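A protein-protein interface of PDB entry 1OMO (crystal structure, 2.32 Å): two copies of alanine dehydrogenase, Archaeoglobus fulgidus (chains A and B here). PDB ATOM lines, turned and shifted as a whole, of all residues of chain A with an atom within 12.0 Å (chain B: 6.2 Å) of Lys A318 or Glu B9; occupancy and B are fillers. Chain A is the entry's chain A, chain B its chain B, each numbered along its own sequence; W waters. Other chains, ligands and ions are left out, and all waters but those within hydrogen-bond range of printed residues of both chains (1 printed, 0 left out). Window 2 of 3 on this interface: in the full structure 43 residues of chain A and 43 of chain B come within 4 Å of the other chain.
The side-chain amino group (NZ) of Lys A318 is in salt-bridge range of the side-chain carboxylate (OE1) of Glu B9, at 3.2 Å.
N of Gln B8 sits at hydrogen-bond distance from O of Phe A319, at 2.9 Å.
Water W1 lies within hydrogen-bond range of OE2 of Glu B9 (2.7 Å) and O of Lys A318 (2.9 Å).
Glu A2 touches none of the printed residues of chain B.
Val A98 touches none of the printed residues of chain B.
Of chain B, only Thr B7 and Glu B9 come within 4 Å of Lys A318.
Printed residues of chain B within 4 Å of Phe A319: Thr B7, Gln B8 and Asp B100.
Printed residues of chain B within 4 Å of Phe A320: Gln B8 (3.6 Å), Glu B9 (3.96 Å) and Asp B100 (3.0 Å).
Of chain A, only Lys A318 and Phe A319 come within 4 Å of Thr B7.
Gln B8 touches just these residues of chain A: Phe A319 (2.9 Å) and Phe A320 (3.6 Å).
No residue of chain A comes within 4 Å of Glu B10.
No residue of chain A comes within 4 Å of Val B11.
Ser B13 touches none of the printed residues of chain A.
Of the printed residues of chain A, Asp B100 touches Phe A319 (3.9 Å) and Phe A320 (3.0 Å).
The nearest printed residue of chain B that does not touch Phe A319 is Glu B9 (4.2 Å).
Among the printed residues, merely in contact across the chains: Lys A318 with Thr B7 (3.5 Å), Phe A319 with Thr B7 (3.8 Å), Phe A319 with Asp B100 (3.9 Å), Phe A320 with Gln B8 (3.6 Å), Phe A320 with Glu B9 (3.96 Å) and Phe A320 with Asp B100 (3.0 Å).
Of the 9 printed residues of chain B, 4 touch a printed residue of chain A.
Hydrophobic or aromatic side chains of chain A within 4 Å of the printed part of chain B: Phe A320.
Among the printed residues, 8 pairs touch across the chains.
Among the printed residues, Asp or Glu carboxylates within 4 Å of a Lys or Arg side-chain nitrogen of the other chain: Lys A318 with Glu B9.
No position is printed for both chains.
Of the 8 pairs that touch across the chains among the printed residues, none has its exchanged pair printed and touching as well.
The side-chain amino group of Lys A318 sits at hydrogen-bond distance from the backbone carbonyl oxygen of Phe A320 (3.1 Å).
OG1 of Thr B7 lies close to OE2 of Glu B9 (3.4 Å).
OE2 of Glu B10 is in hydrogen-bond range of N of Thr B7 (3.0 Å).
The side-chain amide nitrogen (NE2) of Gln B8 lies within hydrogen-bond range of the side-chain carboxylate (OE1) of Glu B12, 3.0 Å away.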
ATOM      1  N   MET A   1       8.148  17.765 -14.481  1.00  0.00           N
ATOM      2  CA  MET A   1       7.563  18.027 -15.831  1.00  0.00           C
ATOM      3  C   MET A   1       6.154  18.554 -15.689  1.00  0.00           C
ATOM      4  O   MET A   1       5.409  18.119 -14.812  1.00  0.00           O
ATOM      5  CB  MET A   1       7.530  16.746 -16.657  1.00  0.00           C
ATOM      6  CG  MET A   1       8.860  16.360 -17.233  1.00  0.00           C
ATOM      7  SD  MET A   1       9.621  17.768 -18.091  1.00  0.00           S
ATOM      8  CE  MET A   1       8.212  18.453 -19.033  1.00  0.00           C
ATOM      9  N   GLU A   2       5.778  19.478 -16.559  1.00  0.00           N
ATOM     10  CA  GLU A   2       4.450  20.067 -16.483  1.00  0.00           C
ATOM     11  C   GLU A   2       3.694  19.984 -17.785  1.00  0.00           C
ATOM     12  O   GLU A   2       4.254  20.258 -18.845  1.00  0.00           O
ATOM     13  CB  GLU A   2       4.550  21.551 -16.108  1.00  0.00           C
ATOM     14  CG  GLU A   2       5.319  21.807 -14.835  1.00  0.00           C
ATOM     15  CD  GLU A   2       4.599  21.254 -13.637  1.00  0.00           C
ATOM     16  OE1 GLU A   2       3.728  21.958 -13.078  1.00  0.00           O
ATOM     17  OE2 GLU A   2       4.893  20.098 -13.268  1.00  0.00           O
ATOM     18  N   THR A   3       2.419  19.622 -17.706  1.00  0.00           N
ATOM     19  CA  THR A   3       1.575  19.593 -18.892  1.00  0.00           C
ATOM     20  C   THR A   3       0.609  20.791 -18.767  1.00  0.00           C
ATOM     21  O   THR A   3      -0.008  21.017 -17.716  1.00  0.00           O
ATOM     22  CB  THR A   3       0.798  18.271 -18.991  1.00  0.00           C
ATOM     23  OG1 THR A   3       1.718  17.201 -19.257  1.00  0.00           O
ATOM     24  CG2 THR A   3      -0.245  18.329 -20.087  1.00  0.00           C
ATOM     25  N   LEU A   4       0.514  21.585 -19.832  1.00  0.00           N
ATOM     26  CA  LEU A   4      -0.358  22.765 -19.864  1.00  0.00           C
ATOM     27  C   LEU A   4      -1.801  22.312 -20.174  1.00  0.00           C
ATOM     28  O   LEU A   4      -2.012  21.451 -21.032  1.00  0.00           O
ATOM     29  CB  LEU A   4       0.154  23.727 -20.949  1.00  0.00           C
ATOM     30  CG  LEU A   4      -0.469  25.089 -21.176  1.00  0.00           C
ATOM     31  CD1 LEU A   4      -0.094  25.992 -20.038  1.00  0.00           C
ATOM     32  CD2 LEU A   4      -0.015  25.652 -22.505  1.00  0.00           C
ATOM     33  N   ILE A   5      -2.773  22.854 -19.444  1.00  0.00           N
ATOM     34  CA  ILE A   5      -4.191  22.529 -19.653  1.00  0.00           C
ATOM     35  C   ILE A   5      -4.870  23.770 -20.226  1.00  0.00           C
ATOM     36  O   ILE A   5      -4.797  24.842 -19.625  1.00  0.00           O
ATOM     37  CB  ILE A   5      -4.875  22.112 -18.316  1.00  0.00           C
ATOM     38  CG1 ILE A   5      -4.156  20.879 -17.741  1.00  0.00           C
ATOM     39  CG2 ILE A   5      -6.338  21.730 -18.544  1.00  0.00           C
ATOM     40  CD1 ILE A   5      -4.074  19.697 -18.720  1.00  0.00           C
ATOM     41  N   LEU A   6      -5.485  23.636 -21.403  1.00  0.00           N
ATOM     42  CA  LEU A   6      -6.162  24.768 -22.043  1.00  0.00           C
ATOM     43  C   LEU A   6      -7.641  24.518 -22.291  1.00  0.00           C
ATOM     44  O   LEU A   6      -8.053  23.514 -22.906  1.00  0.00           O
ATOM     45  CB  LEU A   6      -5.487  25.138 -23.355  1.00  0.00           C
ATOM     46  CG  LEU A   6      -4.117  25.819 -23.301  1.00  0.00           C
ATOM     47  CD1 LEU A   6      -3.660  26.041 -24.718  1.00  0.00           C
ATOM     48  CD2 LEU A   6      -4.162  27.151 -22.557  1.00  0.00           C
ATOM     49  N   PHE A  94       6.781  13.472 -24.665  1.00  0.00           N
ATOM     50  CA  PHE A  94       6.121  14.139 -23.566  1.00  0.00           C
ATOM     51  C   PHE A  94       4.857  14.901 -23.968  1.00  0.00           C
ATOM     52  O   PHE A  94       4.826  15.606 -24.997  1.00  0.00           O
ATOM     53  CB  PHE A  94       7.084  15.103 -22.890  1.00  0.00           C
ATOM     54  CG  PHE A  94       6.520  15.748 -21.646  1.00  0.00           C
ATOM     55  CD1 PHE A  94       6.522  15.069 -20.438  1.00  0.00           C
ATOM     56  CD2 PHE A  94       5.957  17.011 -21.692  1.00  0.00           C
ATOM     57  CE1 PHE A  94       5.970  15.631 -19.293  1.00  0.00           C
ATOM     58  CE2 PHE A  94       5.397  17.597 -20.550  1.00  0.00           C
ATOM     59  CZ  PHE A  94       5.403  16.903 -19.349  1.00  0.00           C
ATOM     60  N   PRO A  95       3.799  14.767 -23.163  1.00  0.00           N
ATOM     61  CA  PRO A  95       2.514  15.445 -23.402  1.00  0.00           C
ATOM     62  C   PRO A  95       2.605  16.892 -22.914  1.00  0.00           C
ATOM     63  O   PRO A  95       2.351  17.189 -21.735  1.00  0.00           O
ATOM     64  CB  PRO A  95       1.516  14.620 -22.586  1.00  0.00           C
ATOM     65  CG  PRO A  95       2.347  14.127 -21.439  1.00  0.00           C
ATOM     66  CD  PRO A  95       3.685  13.763 -22.090  1.00  0.00           C
ATOM     67  N   LEU A  96       2.982  17.768 -23.846  1.00  0.00           N
ATOM     68  CA  LEU A  96       3.150  19.193 -23.632  1.00  0.00           C
ATOM     69  C   LEU A  96       1.848  19.879 -23.224  1.00  0.00           C
ATOM     70  O   LEU A  96       1.840  20.806 -22.406  1.00  0.00           O
ATOM     71  CB  LEU A  96       3.657  19.842 -24.933  1.00  0.00           C
ATOM     72  CG  LEU A  96       5.125  20.060 -25.338  1.00  0.00           C
ATOM     73  CD1 LEU A  96       6.085  19.340 -24.416  1.00  0.00           C
ATOM     74  CD2 LEU A  96       5.307  19.574 -26.776  1.00  0.00           C
ATOM     75  N   ALA A  97       0.736  19.447 -23.803  1.00  0.00           N
ATOM     76  CA  ALA A  97      -0.531  20.103 -23.483  1.00  0.00           C
ATOM     77  C   ALA A  97      -1.749  19.219 -23.769  1.00  0.00           C
ATOM     78  O   ALA A  97      -1.690  18.287 -24.592  1.00  0.00           O
ATOM     79  CB  ALA A  97      -0.647  21.419 -24.301  1.00  0.00           C
ATOM     80  N   VAL A  98      -2.830  19.508 -23.061  1.00  0.00           N
ATOM     81  CA  VAL A  98      -4.108  18.842 -23.242  1.00  0.00           C
ATOM     82  C   VAL A  98      -4.998  20.055 -23.392  1.00  0.00           C
ATOM     83  O   VAL A  98      -5.137  20.842 -22.446  1.00  0.00           O
ATOM     84  CB  VAL A  98      -4.552  18.041 -21.996  1.00  0.00           C
ATOM     85  CG1 VAL A  98      -5.991  17.577 -22.186  1.00  0.00           C
ATOM     86  CG2 VAL A  98      -3.650  16.817 -21.786  1.00  0.00           C
ATOM     87  N   GLY A 314      -3.285  29.555 -19.439  1.00  0.00           N
ATOM     88  CA  GLY A 314      -3.423  28.150 -19.105  1.00  0.00           C
ATOM     89  C   GLY A 314      -3.242  27.857 -17.634  1.00  0.00           C
ATOM     90  O   GLY A 314      -3.249  28.770 -16.816  1.00  0.00           O
ATOM     91  N   SER A 315      -3.132  26.580 -17.295  1.00  0.00           N
ATOM     92  CA  SER A 315      -2.912  26.136 -15.921  1.00  0.00           C
ATOM     93  C   SER A 315      -2.027  24.914 -16.114  1.00  0.00           C
ATOM     94  O   SER A 315      -1.954  24.387 -17.223  1.00  0.00           O
ATOM     95  CB  SER A 315      -4.234  25.787 -15.216  1.00  0.00           C
ATOM     96  OG  SER A 315      -4.875  24.637 -15.753  1.00  0.00           O
ATOM     97  N   LYS A 316      -1.343  24.471 -15.068  1.00  0.00           N
ATOM     98  CA  LYS A 316      -0.433  23.353 -15.222  1.00  0.00           C
ATOM     99  C   LYS A 316      -0.623  22.172 -14.300  1.00  0.00           C
ATOM    100  O   LYS A 316      -0.859  22.346 -13.108  1.00  0.00           O
ATOM    101  CB  LYS A 316       1.000  23.846 -15.054  1.00  0.00           C
ATOM    102  CG  LYS A 316       1.420  24.870 -16.079  1.00  0.00           C
ATOM    103  CD  LYS A 316       2.696  25.585 -15.654  1.00  0.00           C
ATOM    104  CE  LYS A 316       3.261  26.449 -16.775  1.00  0.00           C
ATOM    105  NZ  LYS A 316       3.796  25.601 -17.867  1.00  0.00           N
ATOM    106  N   ILE A 317      -0.478  20.972 -14.852  1.00  0.00           N
ATOM    107  CA  ILE A 317      -0.591  19.775 -14.057  1.00  0.00           C
ATOM    108  C   ILE A 317       0.629  18.867 -14.268  1.00  0.00           C
ATOM    109  O   ILE A 317       1.116  18.721 -15.384  1.00  0.00           O
ATOM    110  CB  ILE A 317      -1.935  19.010 -14.363  1.00  0.00           C
ATOM    111  CG1 ILE A 317      -2.246  18.014 -13.240  1.00  0.00           C
ATOM    112  CG2 ILE A 317      -1.850  18.254 -15.645  1.00  0.00           C
ATOM    113  CD1 ILE A 317      -3.268  18.537 -12.207  1.00  0.00           C
ATOM    114  N   LYS A 318       1.131  18.290 -13.175  1.00  0.00           N
ATOM    115  CA  LYS A 318       2.269  17.363 -13.201  1.00  0.00           C
ATOM    116  C   LYS A 318       1.653  15.963 -13.209  1.00  0.00           C
ATOM    117  O   LYS A 318       1.314  15.410 -12.169  1.00  0.00           O
ATOM    118  CB  LYS A 318       3.130  17.557 -11.941  1.00  0.00           C
ATOM    119  CG  LYS A 318       4.427  16.720 -11.881  1.00  0.00           C
ATOM    120  CD  LYS A 318       5.134  16.876 -10.519  1.00  0.00           C
ATOM    121  CE  LYS A 318       4.788  15.729  -9.551  1.00  0.00           C
ATOM    122  NZ  LYS A 318       5.794  14.626  -9.664  1.00  0.00           N
ATOM    123  N   PHE A 319       1.491  15.400 -14.390  1.00  0.00           N
ATOM    124  CA  PHE A 319       0.888  14.095 -14.518  1.00  0.00           C
ATOM    125  C   PHE A 319       1.709  12.929 -14.026  1.00  0.00           C
ATOM    126  O   PHE A 319       1.161  11.972 -13.494  1.00  0.00           O
ATOM    127  CB  PHE A 319       0.526  13.825 -15.983  1.00  0.00           C
ATOM    128  CG  PHE A 319      -0.819  14.372 -16.404  1.00  0.00           C
ATOM    129  CD1 PHE A 319      -0.909  15.378 -17.355  1.00  0.00           C
ATOM    130  CD2 PHE A 319      -1.989  13.867 -15.860  1.00  0.00           C
ATOM    131  CE1 PHE A 319      -2.160  15.867 -17.754  1.00  0.00           C
ATOM    132  CE2 PHE A 319      -3.222  14.349 -16.253  1.00  0.00           C
ATOM    133  CZ  PHE A 319      -3.312  15.341 -17.196  1.00  0.00           C
ATOM    134  N   PHE A 320       3.020  12.993 -14.209  1.00  0.00           N
ATOM    135  CA  PHE A 320       3.881  11.864 -13.859  1.00  0.00           C
ATOM    136  C   PHE A 320       4.815  12.053 -12.677  1.00  0.00           C
ATOM    137  O   PHE A 320       5.042  13.219 -12.308  1.00  0.00           O
ATOM    138  CB  PHE A 320       4.709  11.477 -15.083  1.00  0.00           C
ATOM    139  CG  PHE A 320       3.938  11.529 -16.361  1.00  0.00           C
ATOM    140  CD1 PHE A 320       4.219  12.497 -17.313  1.00  0.00           C
ATOM    141  CD2 PHE A 320       2.893  10.635 -16.587  1.00  0.00           C
ATOM    142  CE1 PHE A 320       3.476  12.587 -18.474  1.00  0.00           C
ATOM    143  CE2 PHE A 320       2.140  10.717 -17.746  1.00  0.00           C
ATOM    144  CZ  PHE A 320       2.437  11.705 -18.696  1.00  0.00           C
ATOM    145  N   THR B   7      -3.520  12.486 -11.442  1.00  0.00           N
ATOM    146  CA  THR B   7      -2.064  12.356 -11.550  1.00  0.00           C
ATOM    147  C   THR B   7      -1.678  10.924 -11.262  1.00  0.00           C
ATOM    148  O   THR B   7      -2.478  10.162 -10.713  1.00  0.00           O
ATOM    149  CB  THR B   7      -1.337  13.195 -10.498  1.00  0.00           C
ATOM    150  OG1 THR B   7      -1.697  12.700  -9.199  1.00  0.00           O
ATOM    151  CG2 THR B   7      -1.696  14.673 -10.611  1.00  0.00           C
ATOM    152  N   GLN B   8      -0.434  10.579 -11.580  1.00  0.00           N
ATOM    153  CA  GLN B   8       0.066   9.227 -11.353  1.00  0.00           C
ATOM    154  C   GLN B   8       0.049   8.826  -9.877  1.00  0.00           C
ATOM    155  O   GLN B   8      -0.200   7.678  -9.521  1.00  0.00           O
ATOM    156  CB  GLN B   8       1.482   9.108 -11.894  1.00  0.00           C
ATOM    157  CG  GLN B   8       2.074   7.728 -11.622  1.00  0.00           C
ATOM    158  CD  GLN B   8       3.520   7.604 -12.077  1.00  0.00           C
ATOM    159  OE1 GLN B   8       4.062   8.509 -12.704  1.00  0.00           O
ATOM    160  NE2 GLN B   8       4.142   6.474 -11.768  1.00  0.00           N
ATOM    161  N   GLU B   9       0.294   9.789  -9.011  1.00  0.00           N
ATOM    162  CA  GLU B   9       0.303   9.535  -7.590  1.00  0.00           C
ATOM    163  C   GLU B   9      -1.102   9.250  -7.108  1.00  0.00           C
ATOM    164  O   GLU B   9      -1.324   8.418  -6.217  1.00  0.00           O
ATOM    165  CB  GLU B   9       0.866  10.754  -6.874  1.00  0.00           C
ATOM    166  CG  GLU B   9       2.324  11.014  -7.244  1.00  0.00           C
ATOM    167  CD  GLU B   9       2.555  11.885  -8.516  1.00  0.00           C
ATOM    168  OE1 GLU B   9       3.692  12.407  -8.680  1.00  0.00           O
ATOM    169  OE2 GLU B   9       1.631  12.056  -9.348  1.00  0.00           O
ATOM    170  N   GLU B  10      -2.063   9.974  -7.675  1.00  0.00           N
ATOM    171  CA  GLU B  10      -3.447   9.764  -7.293  1.00  0.00           C
ATOM    172  C   GLU B  10      -3.928   8.423  -7.821  1.00  0.00           C
ATOM    173  O   GLU B  10      -4.525   7.673  -7.071  1.00  0.00           O
ATOM    174  CB  GLU B  10      -4.305  10.909  -7.818  1.00  0.00           C
ATOM    175  CG  GLU B  10      -4.114  12.217  -7.039  1.00  0.00           C
ATOM    176  CD  GLU B  10      -4.714  13.407  -7.757  1.00  0.00           C
ATOM    177  OE1 GLU B  10      -4.894  14.469  -7.127  1.00  0.00           O
ATOM    178  OE2 GLU B  10      -4.992  13.270  -8.964  1.00  0.00           O
ATOM    179  N   VAL B  11      -3.639   8.102  -9.090  1.00  0.00           N
ATOM    180  CA  VAL B  11      -4.099   6.833  -9.666  1.00  0.00           C
ATOM    181  C   VAL B  11      -3.544   5.682  -8.871  1.00  0.00           C
ATOM    182  O   VAL B  11      -4.243   4.690  -8.659  1.00  0.00           O
ATOM    183  CB  VAL B  11      -3.667   6.632 -11.147  1.00  0.00           C
ATOM    184  CG1 VAL B  11      -4.048   5.238 -11.625  1.00  0.00           C
ATOM    185  CG2 VAL B  11      -4.349   7.646 -12.038  1.00  0.00           C
ATOM    186  N   GLU B  12      -2.283   5.813  -8.432  1.00  0.00           N
ATOM    187  CA  GLU B  12      -1.633   4.750  -7.682  1.00  0.00           C
ATOM    188  C   GLU B  12      -2.369   4.422  -6.400  1.00  0.00           C
ATOM    189  O   GLU B  12      -2.359   3.286  -5.942  1.00  0.00           O
ATOM    190  CB  GLU B  12      -0.164   5.112  -7.410  1.00  0.00           C
ATOM    191  CG  GLU B  12       0.746   4.970  -8.652  1.00  0.00           C
ATOM    192  CD  GLU B  12       2.154   5.506  -8.428  1.00  0.00           C
ATOM    193  OE1 GLU B  12       3.071   5.230  -9.246  1.00  0.00           O
ATOM    194  OE2 GLU B  12       2.356   6.219  -7.427  1.00  0.00           O
ATOM    195  N   SER B  13      -3.023   5.417  -5.827  1.00  0.00           N
ATOM    196  CA  SER B  13      -3.781   5.199  -4.609  1.00  0.00           C
ATOM    197  C   SER B  13      -5.232   4.790  -4.918  1.00  0.00           C
ATOM    198  O   SER B  13      -6.023   4.572  -3.997  1.00  0.00           O
ATOM    199  CB  SER B  13      -3.815   6.471  -3.773  1.00  0.00           C
ATOM    200  OG  SER B  13      -4.655   7.439  -4.400  1.00  0.00           O
ATOM    201  N   LEU B  14      -5.592   4.667  -6.196  1.00  0.00           N
ATOM    202  CA  LEU B  14      -6.987   4.333  -6.516  1.00  0.00           C
ATOM    203  C   LEU B  14      -7.268   2.951  -7.068  1.00  0.00           C
ATOM    204  O   LEU B  14      -8.414   2.610  -7.327  1.00  0.00           O
ATOM    205  CB  LEU B  14      -7.569   5.386  -7.453  1.00  0.00           C
ATOM    206  CG  LEU B  14      -7.617   6.845  -6.939  1.00  0.00           C
ATOM    207  CD1 LEU B  14      -7.840   7.815  -8.105  1.00  0.00           C
ATOM    208  CD2 LEU B  14      -8.724   6.994  -5.915  1.00  0.00           C
ATOM    209  N   ASP B 100      -3.412   9.758 -15.685  1.00  0.00           N
ATOM    210  CA  ASP B 100      -2.161   9.087 -15.971  1.00  0.00           C
ATOM    211  C   ASP B 100      -2.424   7.617 -16.201  1.00  0.00           C
ATOM    212  O   ASP B 100      -3.219   7.014 -15.491  1.00  0.00           O
ATOM    213  CB  ASP B 100      -1.174   9.211 -14.820  1.00  0.00           C
ATOM    214  CG  ASP B 100       0.024   8.322 -15.025  1.00  0.00           C
ATOM    215  OD1 ASP B 100       0.802   8.553 -15.981  1.00  0.00           O
ATOM    216  OD2 ASP B 100       0.165   7.356 -14.255  1.00  0.00           O
HETATM  217  O   HOH W   1       2.061  14.730  -9.450  1.00  0.00           O
